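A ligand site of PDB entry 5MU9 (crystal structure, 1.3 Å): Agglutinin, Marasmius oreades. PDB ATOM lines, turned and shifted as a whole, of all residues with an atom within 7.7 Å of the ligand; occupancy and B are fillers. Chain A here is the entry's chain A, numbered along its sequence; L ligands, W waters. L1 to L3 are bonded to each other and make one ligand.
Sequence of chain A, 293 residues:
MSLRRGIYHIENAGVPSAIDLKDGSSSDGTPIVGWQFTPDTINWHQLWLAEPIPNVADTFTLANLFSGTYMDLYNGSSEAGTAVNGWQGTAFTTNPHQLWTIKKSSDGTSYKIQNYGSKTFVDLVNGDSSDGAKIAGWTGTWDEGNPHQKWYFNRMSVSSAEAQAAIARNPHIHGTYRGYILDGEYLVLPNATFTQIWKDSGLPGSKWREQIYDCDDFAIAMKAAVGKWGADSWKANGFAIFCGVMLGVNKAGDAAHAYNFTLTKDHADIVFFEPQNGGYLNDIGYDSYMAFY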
ATOM      1  N   ASP A  28      21.224   8.745  -7.079  1.00  0.00           N
ATOM      2  CA  ASP A  28      20.155   9.706  -7.305  1.00  0.00           C
ATOM      3  C   ASP A  28      19.935   9.870  -8.773  1.00  0.00           C
ATOM      4  O   ASP A  28      20.870  10.119  -9.533  1.00  0.00           O
ATOM      5  CB  ASP A  28      20.489  11.086  -6.649  1.00  0.00           C
ATOM      6  CG  ASP A  28      20.527  11.057  -5.115  1.00  0.00           C
ATOM      7  OD1 ASP A  28      19.819  10.184  -4.532  1.00  0.00           O
ATOM      8  OD2 ASP A  28      21.021  12.032  -4.487  1.00  0.00           O
ATOM      9  N   GLY A  29      18.677   9.918  -9.201  1.00  0.00           N
ATOM     10  CA  GLY A  29      18.337  10.120 -10.594  1.00  0.00           C
ATOM     11  C   GLY A  29      18.298   8.895 -11.463  1.00  0.00           C
ATOM     12  O   GLY A  29      18.089   8.988 -12.657  1.00  0.00           O
ATOM     13  N   MET A  71      10.816   6.595  -4.942  1.00  0.00           N
ATOM     14  CA  MET A  71      10.232   7.158  -6.186  1.00  0.00           C
ATOM     15  C   MET A  71      10.069   8.667  -6.117  1.00  0.00           C
ATOM     16  O   MET A  71       9.467   9.177  -5.101  1.00  0.00           O
ATOM     17  CB  MET A  71       8.901   6.447  -6.423  1.00  0.00           C
ATOM     18  CG  MET A  71       8.253   6.851  -7.737  1.00  0.00           C
ATOM     19  SD  MET A  71       6.645   6.111  -8.059  1.00  0.00           S
ATOM     20  CE  MET A  71       7.114   4.443  -8.279  1.00  0.00           C
ATOM     21  N   ASP A  72      10.653   9.402  -7.067  1.00  0.00           N
ATOM     22  CA  ASP A  72      10.793  10.831  -6.988  1.00  0.00           C
ATOM     23  C   ASP A  72      10.428  11.417  -8.353  1.00  0.00           C
ATOM     24  O   ASP A  72      11.008  11.017  -9.375  1.00  0.00           O
ATOM     25  CB  ASP A  72      12.245  11.135  -6.571  1.00  0.00           C
ATOM     26  CG  ASP A  72      12.609  12.565  -6.432  1.00  0.00           C
ATOM     27  OD1 ASP A  72      12.518  13.293  -7.408  1.00  0.00           O
ATOM     28  OD2 ASP A  72      12.854  13.054  -5.266  1.00  0.00           O
ATOM     29  N   LEU A  73       9.539  12.407  -8.335  1.00  0.00           N
ATOM     30  CA  LEU A  73       9.174  13.149  -9.548  1.00  0.00           C
ATOM     31  C   LEU A  73      10.174  14.308  -9.671  1.00  0.00           C
ATOM     32  O   LEU A  73      10.197  15.213  -8.813  1.00  0.00           O
ATOM     33  CB  LEU A  73       7.778  13.702  -9.433  1.00  0.00           C
ATOM     34  CG  LEU A  73       7.256  14.498 -10.641  1.00  0.00           C
ATOM     35  CD1 LEU A  73       7.152  13.590 -11.881  1.00  0.00           C
ATOM     36  CD2 LEU A  73       5.944  15.206 -10.305  1.00  0.00           C
ATOM     37  N   TYR A  74      10.928  14.343 -10.760  1.00  0.00           N
ATOM     38  CA  TYR A  74      12.060  15.242 -10.887  1.00  0.00           C
ATOM     39  C   TYR A  74      11.679  16.684 -10.768  1.00  0.00           C
ATOM     40  O   TYR A  74      10.983  17.227 -11.631  1.00  0.00           O
ATOM     41  CB  TYR A  74      12.846  14.907 -12.133  1.00  0.00           C
ATOM     42  CG  TYR A  74      14.182  15.592 -12.244  1.00  0.00           C
ATOM     43  CD1 TYR A  74      15.188  15.342 -11.317  1.00  0.00           C
ATOM     44  CD2 TYR A  74      14.436  16.571 -13.248  1.00  0.00           C
ATOM     45  CE1 TYR A  74      16.404  16.028 -11.407  1.00  0.00           C
ATOM     46  CE2 TYR A  74      15.625  17.211 -13.311  1.00  0.00           C
ATOM     47  CZ  TYR A  74      16.638  16.926 -12.340  1.00  0.00           C
ATOM     48  OH  TYR A  74      17.841  17.574 -12.436  1.00  0.00           O
ATOM     49  N   ASN A  75      12.258  17.346  -9.757  1.00  0.00           N
ATOM     50  CA  ASN A  75      11.998  18.783  -9.429  1.00  0.00           C
ATOM     51  C   ASN A  75      10.498  19.072  -9.255  1.00  0.00           C
ATOM     52  O   ASN A  75      10.075  20.244  -9.199  1.00  0.00           O
ATOM     53  CB  ASN A  75      12.641  19.648 -10.459  1.00  0.00           C
ATOM     54  CG  ASN A  75      14.096  19.811 -10.243  1.00  0.00           C
ATOM     55  OD1 ASN A  75      14.584  19.857  -9.128  1.00  0.00           O
ATOM     56  ND2 ASN A  75      14.820  19.873 -11.339  1.00  0.00           N
ATOM     57  N   GLY A  76       9.697  18.017  -9.013  1.00  0.00           N
ATOM     58  CA  GLY A  76       8.261  18.208  -8.754  1.00  0.00           C
ATOM     59  C   GLY A  76       7.486  18.757  -9.958  1.00  0.00           C
ATOM     60  O   GLY A  76       6.383  19.283  -9.791  1.00  0.00           O
ATOM     61  N   SER A  77       8.031  18.709 -11.164  1.00  0.00           N
ATOM     62  CA  SER A  77       7.367  19.422 -12.266  1.00  0.00           C
ATOM     63  C   SER A  77       6.073  18.775 -12.672  1.00  0.00           C
ATOM     64  O   SER A  77       5.985  17.564 -12.766  1.00  0.00           O
ATOM     65  CB  SER A  77       8.305  19.485 -13.475  1.00  0.00           C
ATOM     66  OG  SER A  77       7.664  20.082 -14.588  1.00  0.00           O
ATOM     67  N   THR A  82       7.777  14.462 -17.394  1.00  0.00           N
ATOM     68  CA  THR A  82       8.753  14.642 -16.302  1.00  0.00           C
ATOM     69  C   THR A  82       9.290  13.301 -15.834  1.00  0.00           C
ATOM     70  O   THR A  82       8.506  12.386 -15.575  1.00  0.00           O
ATOM     71  CB  THR A  82       8.134  15.524 -15.178  1.00  0.00           C
ATOM     72  OG1 THR A  82       7.845  16.836 -15.640  1.00  0.00           O
ATOM     73  CG2 THR A  82       9.069  15.671 -13.954  1.00  0.00           C
ATOM     74  N   ALA A  83      10.588  13.233 -15.650  1.00  0.00           N
ATOM     75  CA  ALA A  83      11.199  12.031 -15.154  1.00  0.00           C
ATOM     76  C   ALA A  83      10.717  11.535 -13.809  1.00  0.00           C
ATOM     77  O   ALA A  83      10.530  12.339 -12.894  1.00  0.00           O
ATOM     78  CB  ALA A  83      12.750  12.204 -15.131  1.00  0.00           C
ATOM     79  N   ASN A  85      12.263   8.894 -11.080  1.00  0.00           N
ATOM     80  CA  ASN A  85      13.530   8.335 -10.783  1.00  0.00           C
ATOM     81  C   ASN A  85      13.565   7.855  -9.323  1.00  0.00           C
ATOM     82  O   ASN A  85      12.857   8.398  -8.476  1.00  0.00           O
ATOM     83  CB  ASN A  85      14.678   9.384 -10.927  1.00  0.00           C
ATOM     84  CG  ASN A  85      14.796  10.056 -12.292  1.00  0.00           C
ATOM     85  OD1 ASN A  85      14.809   9.376 -13.292  1.00  0.00           O
ATOM     86  ND2 ASN A  85      14.860  11.353 -12.262  1.00  0.00           N
ATOM     87  N   GLY A  86      14.570   7.023  -9.038  1.00  0.00           N
ATOM     88  CA  GLY A  86      14.900   6.827  -7.623  1.00  0.00           C
ATOM     89  C   GLY A  86      15.759   7.948  -7.107  1.00  0.00           C
ATOM     90  O   GLY A  86      16.668   8.454  -7.797  1.00  0.00           O
ATOM     91  N   TRP A  87      15.587   8.294  -5.816  1.00  0.00           N
ATOM     92  CA  TRP A  87      16.315   9.403  -5.225  1.00  0.00           C
ATOM     93  C   TRP A  87      16.383   9.182  -3.699  1.00  0.00           C
ATOM     94  O   TRP A  87      15.416   8.652  -3.078  1.00  0.00           O
ATOM     95  CB  TRP A  87      15.586  10.720  -5.514  1.00  0.00           C
ATOM     96  CG  TRP A  87      16.488  11.962  -5.509  1.00  0.00           C
ATOM     97  CD1 TRP A  87      16.989  12.607  -4.436  1.00  0.00           C
ATOM     98  CD2 TRP A  87      16.949  12.632  -6.641  1.00  0.00           C
ATOM     99  NE1 TRP A  87      17.849  13.601  -4.861  1.00  0.00           N
ATOM    100  CE2 TRP A  87      17.825  13.660  -6.213  1.00  0.00           C
ATOM    101  CE3 TRP A  87      16.775  12.425  -8.018  1.00  0.00           C
ATOM    102  CZ2 TRP A  87      18.455  14.503  -7.087  1.00  0.00           C
ATOM    103  CZ3 TRP A  87      17.449  13.299  -8.950  1.00  0.00           C
ATOM    104  CH2 TRP A  87      18.306  14.313  -8.462  1.00  0.00           C
ATOM    105  N   GLN A  88      17.472   9.643  -3.091  1.00  0.00           N
ATOM    106  CA  GLN A  88      17.580   9.501  -1.677  1.00  0.00           C
ATOM    107  C   GLN A  88      16.414  10.212  -0.954  1.00  0.00           C
ATOM    108  O   GLN A  88      15.950  11.254  -1.372  1.00  0.00           O
ATOM    109  CB  GLN A  88      18.896   9.998  -1.127  1.00  0.00           C
ATOM    110  CG  GLN A  88      19.176  11.472  -1.387  1.00  0.00           C
ATOM    111  CD  GLN A  88      20.478  11.904  -0.826  1.00  0.00           C
ATOM    112  OE1 GLN A  88      20.697  11.960   0.393  1.00  0.00           O
ATOM    113  NE2 GLN A  88      21.379  12.217  -1.717  1.00  0.00           N
ATOM    114  N   GLY A  89      15.967   9.606   0.168  1.00  0.00           N
ATOM    115  CA  GLY A  89      14.882  10.209   0.933  1.00  0.00           C
ATOM    116  C   GLY A  89      14.658   9.505   2.282  1.00  0.00           C
ATOM    117  O   GLY A  89      15.567   8.796   2.736  1.00  0.00           O
ATOM    118  N   THR A  90      13.526   9.738   2.896  1.00  0.00           N
ATOM    119  CA  THR A  90      13.133   9.009   4.124  1.00  0.00           C
ATOM    120  C   THR A  90      11.635   8.693   4.097  1.00  0.00           C
ATOM    121  O   THR A  90      10.861   9.286   3.284  1.00  0.00           O
ATOM    122  CB  THR A  90      13.401   9.851   5.401  1.00  0.00           C
ATOM    123  OG1 THR A  90      12.676  11.100   5.237  1.00  0.00           O
ATOM    124  CG2 THR A  90      14.937  10.126   5.514  1.00  0.00           C
ATOM    125  N   THR A  93       9.063  11.659   4.765  1.00  0.00           N
ATOM    126  CA  THR A  93       9.516  12.936   4.265  1.00  0.00           C
ATOM    127  C   THR A  93       8.327  13.893   4.006  1.00  0.00           C
ATOM    128  O   THR A  93       7.217  13.379   3.664  1.00  0.00           O
ATOM    129  CB  THR A  93      10.243  12.747   2.874  1.00  0.00           C
ATOM    130  OG1 THR A  93      10.875  13.984   2.489  1.00  0.00           O
ATOM    131  CG2 THR A  93       9.416  12.199   1.776  1.00  0.00           C
ATOM    132  N   THR A  94       8.622  15.207   4.072  1.00  0.00           N
ATOM    133  CA  THR A  94       7.659  16.235   3.705  1.00  0.00           C
ATOM    134  C   THR A  94       7.973  16.667   2.236  1.00  0.00           C
ATOM    135  O   THR A  94       7.280  17.524   1.701  1.00  0.00           O
ATOM    136  CB  THR A  94       7.666  17.408   4.629  1.00  0.00           C
ATOM    137  OG1 THR A  94       8.968  17.922   4.616  1.00  0.00           O
ATOM    138  CG2 THR A  94       7.303  17.045   6.032  1.00  0.00           C
ATOM    139  N   ASN A  95       8.942  16.058   1.551  1.00  0.00           N
ATOM    140  CA  ASN A  95       9.298  16.502   0.198  1.00  0.00           C
ATOM    141  C   ASN A  95       8.184  15.985  -0.749  1.00  0.00           C
ATOM    142  O   ASN A  95       8.089  14.808  -0.992  1.00  0.00           O
ATOM    143  CB  ASN A  95      10.576  15.797  -0.241  1.00  0.00           C
ATOM    144  CG  ASN A  95      11.043  16.183  -1.633  1.00  0.00           C
ATOM    145  OD1 ASN A  95      10.327  16.841  -2.410  1.00  0.00           O
ATOM    146  ND2 ASN A  95      12.227  15.749  -1.976  1.00  0.00           N
ATOM    147  N   PRO A  96       7.425  16.905  -1.393  1.00  0.00           N
ATOM    148  CA  PRO A  96       6.313  16.419  -2.264  1.00  0.00           C
ATOM    149  C   PRO A  96       6.777  15.640  -3.482  1.00  0.00           C
ATOM    150  O   PRO A  96       5.954  14.946  -4.074  1.00  0.00           O
ATOM    151  CB  PRO A  96       5.546  17.707  -2.576  1.00  0.00           C
ATOM    152  CG  PRO A  96       6.452  18.799  -2.311  1.00  0.00           C
ATOM    153  CD  PRO A  96       7.446  18.392  -1.271  1.00  0.00           C
ATOM    154  N   HIS A  97       8.014  15.839  -3.896  1.00  0.00           N
ATOM    155  CA  HIS A  97       8.525  15.086  -5.008  1.00  0.00           C
ATOM    156  C   HIS A  97       8.451  13.550  -4.789  1.00  0.00           C
ATOM    157  O   HIS A  97       8.460  12.781  -5.731  1.00  0.00           O
ATOM    158  CB  HIS A  97       9.978  15.434  -5.361  1.00  0.00           C
ATOM    159  CG  HIS A  97      10.220  16.890  -5.538  1.00  0.00           C
ATOM    160  ND1 HIS A  97      11.483  17.369  -5.769  1.00  0.00           N
ATOM    161  CD2 HIS A  97       9.386  17.956  -5.593  1.00  0.00           C
ATOM    162  CE1 HIS A  97      11.420  18.685  -5.887  1.00  0.00           C
ATOM    163  NE2 HIS A  97      10.156  19.038  -5.841  1.00  0.00           N
ATOM    164  N   GLN A  98       8.428  13.168  -3.493  1.00  0.00           N
ATOM    165  CA  GLN A  98       8.500  11.788  -3.085  1.00  0.00           C
ATOM    166  C   GLN A  98       7.175  11.266  -2.453  1.00  0.00           C
ATOM    167  O   GLN A  98       7.125  10.219  -1.864  1.00  0.00           O
ATOM    168  CB  GLN A  98       9.683  11.535  -2.131  1.00  0.00           C
ATOM    169  CG  GLN A  98      10.995  11.682  -2.915  1.00  0.00           C
ATOM    170  CD  GLN A  98      12.236  11.607  -2.022  1.00  0.00           C
ATOM    171  OE1 GLN A  98      12.120  11.282  -0.805  1.00  0.00           O
ATOM    172  NE2 GLN A  98      13.358  11.920  -2.593  1.00  0.00           N
HETATM  173  C1  LIG L   1      14.792  19.267  -1.788  1.00  0.00           C
HETATM  174  C2  LIG L   1      15.694  20.033  -0.760  1.00  0.00           C
HETATM  175  C3  LIG L   1      16.214  21.343  -1.372  1.00  0.00           C
HETATM  176  C4  LIG L   1      15.035  22.174  -1.855  1.00  0.00           C
HETATM  177  C5  LIG L   1      14.202  21.327  -2.861  1.00  0.00           C
HETATM  178  C6  LIG L   1      12.939  22.083  -3.224  1.00  0.00           C
HETATM  179  O1  LIG L   1      16.870  19.259  -0.471  1.00  0.00           O
HETATM  180  O2  LIG L   1      17.020  22.107  -0.431  1.00  0.00           O
HETATM  181  O3  LIG L   1      14.226  22.551  -0.744  1.00  0.00           O
HETATM  182  O4  LIG L   1      13.712  20.129  -2.214  1.00  0.00           O
HETATM  183  C1  LG2 L   2      15.123  18.545  -5.132  1.00  0.00           C
HETATM  184  C2  LG2 L   2      14.912  17.993  -3.769  1.00  0.00           C
HETATM  185  C3  LG2 L   2      15.552  16.580  -3.687  1.00  0.00           C
HETATM  186  C4  LG2 L   2      14.908  15.722  -4.859  1.00  0.00           C
HETATM  187  C5  LG2 L   2      15.223  16.442  -6.164  1.00  0.00           C
HETATM  188  C6  LG2 L   2      14.749  15.734  -7.396  1.00  0.00           C
HETATM  189  O1  LG2 L   2      16.483  18.824  -5.485  1.00  0.00           O
HETATM  190  O2  LG2 L   2      15.636  18.881  -2.850  1.00  0.00           O
HETATM  191  O3  LG2 L   2      15.280  16.102  -2.407  1.00  0.00           O
HETATM  192  O4  LG2 L   2      13.528  15.511  -4.618  1.00  0.00           O
HETATM  193  O5  LG2 L   2      14.608  17.692  -6.134  1.00  0.00           O
HETATM  194  O6  LG2 L   2      13.335  15.775  -7.574  1.00  0.00           O
HETATM  195  C1  LG3 L   3      15.874  14.879  -1.972  1.00  0.00           C
HETATM  196  C2  LG3 L   3      15.666  14.742  -0.487  1.00  0.00           C
HETATM  197  C3  LG3 L   3      16.530  15.806   0.261  1.00  0.00           C
HETATM  198  C4  LG3 L   3      17.948  15.762  -0.171  1.00  0.00           C
HETATM  199  C5  LG3 L   3      18.094  15.877  -1.660  1.00  0.00           C
HETATM  200  C6  LG3 L   3      19.447  15.627  -2.256  1.00  0.00           C
HETATM  201  O1  LG3 L   3      14.315  14.876  -0.144  1.00  0.00           O
HETATM  202  O2  LG3 L   3      16.248  15.582   1.687  1.00  0.00           O
HETATM  203  O3  LG3 L   3      18.505  14.554   0.335  1.00  0.00           O
HETATM  204  O4  LG3 L   3      17.246  14.872  -2.293  1.00  0.00           O
HETATM  205  O5  LG3 L   3      19.508  15.776  -3.672  1.00  0.00           O
HETATM  206  O   HOH W   1      21.492  14.539  -4.888  1.00  0.00           O
HETATM  207  O   HOH W   2      12.999  12.976   1.174  1.00  0.00           O
HETATM  208  O   HOH W   3      16.560  13.059   2.904  1.00  0.00           O
HETATM  209  O   HOH W   4      11.202  19.481  -2.568  1.00  0.00           O
HETATM  210  O   HOH W   5      18.886  18.457  -4.039  1.00  0.00           O
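OD1 of Asp 72 lies within hydrogen-bond range of O6 of LG2 L2 (2.6 Å).
An oxygen (O6) of LG2 L2 lies within hydrogen-bond range of the backbone NH of Asn 75 (2.9 Å).
The side-chain amide nitrogen (ND2) of Asn 95 lies within hydrogen-bond range of an oxygen (O1) of LG3 L3 (2.9 Å).
The indole nitrogen (NE1) of Trp 87 lies within hydrogen-bond range of an oxygen (O4) of LG3 L3, at 2.9 Å.
ND1 of His 97 sits at hydrogen-bond distance from O4 of LG2 L2 (3.0 Å).
An oxygen (O3) of LG3 L3 sits at hydrogen-bond distance from the side-chain amide oxygen (OE1) of Gln 88, 3.4 Å away.
An oxygen (O6) of LG2 L2 lies within hydrogen-bond range of the backbone carbonyl oxygen (O) of Leu 73, at 3.4 Å.
The side-chain amide nitrogen (NE2) of Gln 98 lies within hydrogen-bond range of the side-chain carboxylate (OD2) of Asp 72 (2.9 Å).
The backbone NH (N) of Asp 72 lies within hydrogen-bond range of the backbone carbonyl oxygen (O) of Asn 85, at 2.8 Å.
OD1 of Asn 95 sits at hydrogen-bond distance from N of His 97 (2.9 Å).
The backbone NH (N) of Asn 95 is in hydrogen-bond range of the side-chain hydroxyl (OG1) of Thr 93 (3.0 Å).
O of His 97 sits at hydrogen-bond distance from N of Leu 73 (2.8 Å).
O of Gln 88 is in hydrogen-bond range of NE2 of Gln 98 (2.9 Å).
The side-chain amide nitrogen of Gln 88 lies within hydrogen-bond range of the side-chain carboxylate of Asp 28.
O of Ala 83 is in hydrogen-bond range of N of Tyr 74 (3.0 Å).
CA of Tyr 74 touches O6 of LG2 L2, at 3.6 Å.
Gln 98 touches the ligand.
Within 4 Å of the ligand: Asp 72, Leu 73, Tyr 74, Asn 75, Trp 87, Gln 88, Asn 95, His 97 and Gln 98.
The nearest printed residue that does not touch the ligand is Asp 28 (4.1 Å).
Water W4 lies within hydrogen-bond range of O4 of LIG L1, OD1 of Asn 95 and NE2 of His 97.
Water W1 lies within hydrogen-bond range of the side-chain carboxylate of Asp 28 (2.6 Å) and an oxygen (O5) of LG3 L3 (2.6 Å).
Water W2 lies within hydrogen-bond range of an oxygen (O1) of LG3 L3 (2.7 Å), the side-chain hydroxyl of Thr 93 (2.7 Å) and the side-chain amide oxygen of Gln 98 (2.7 Å).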
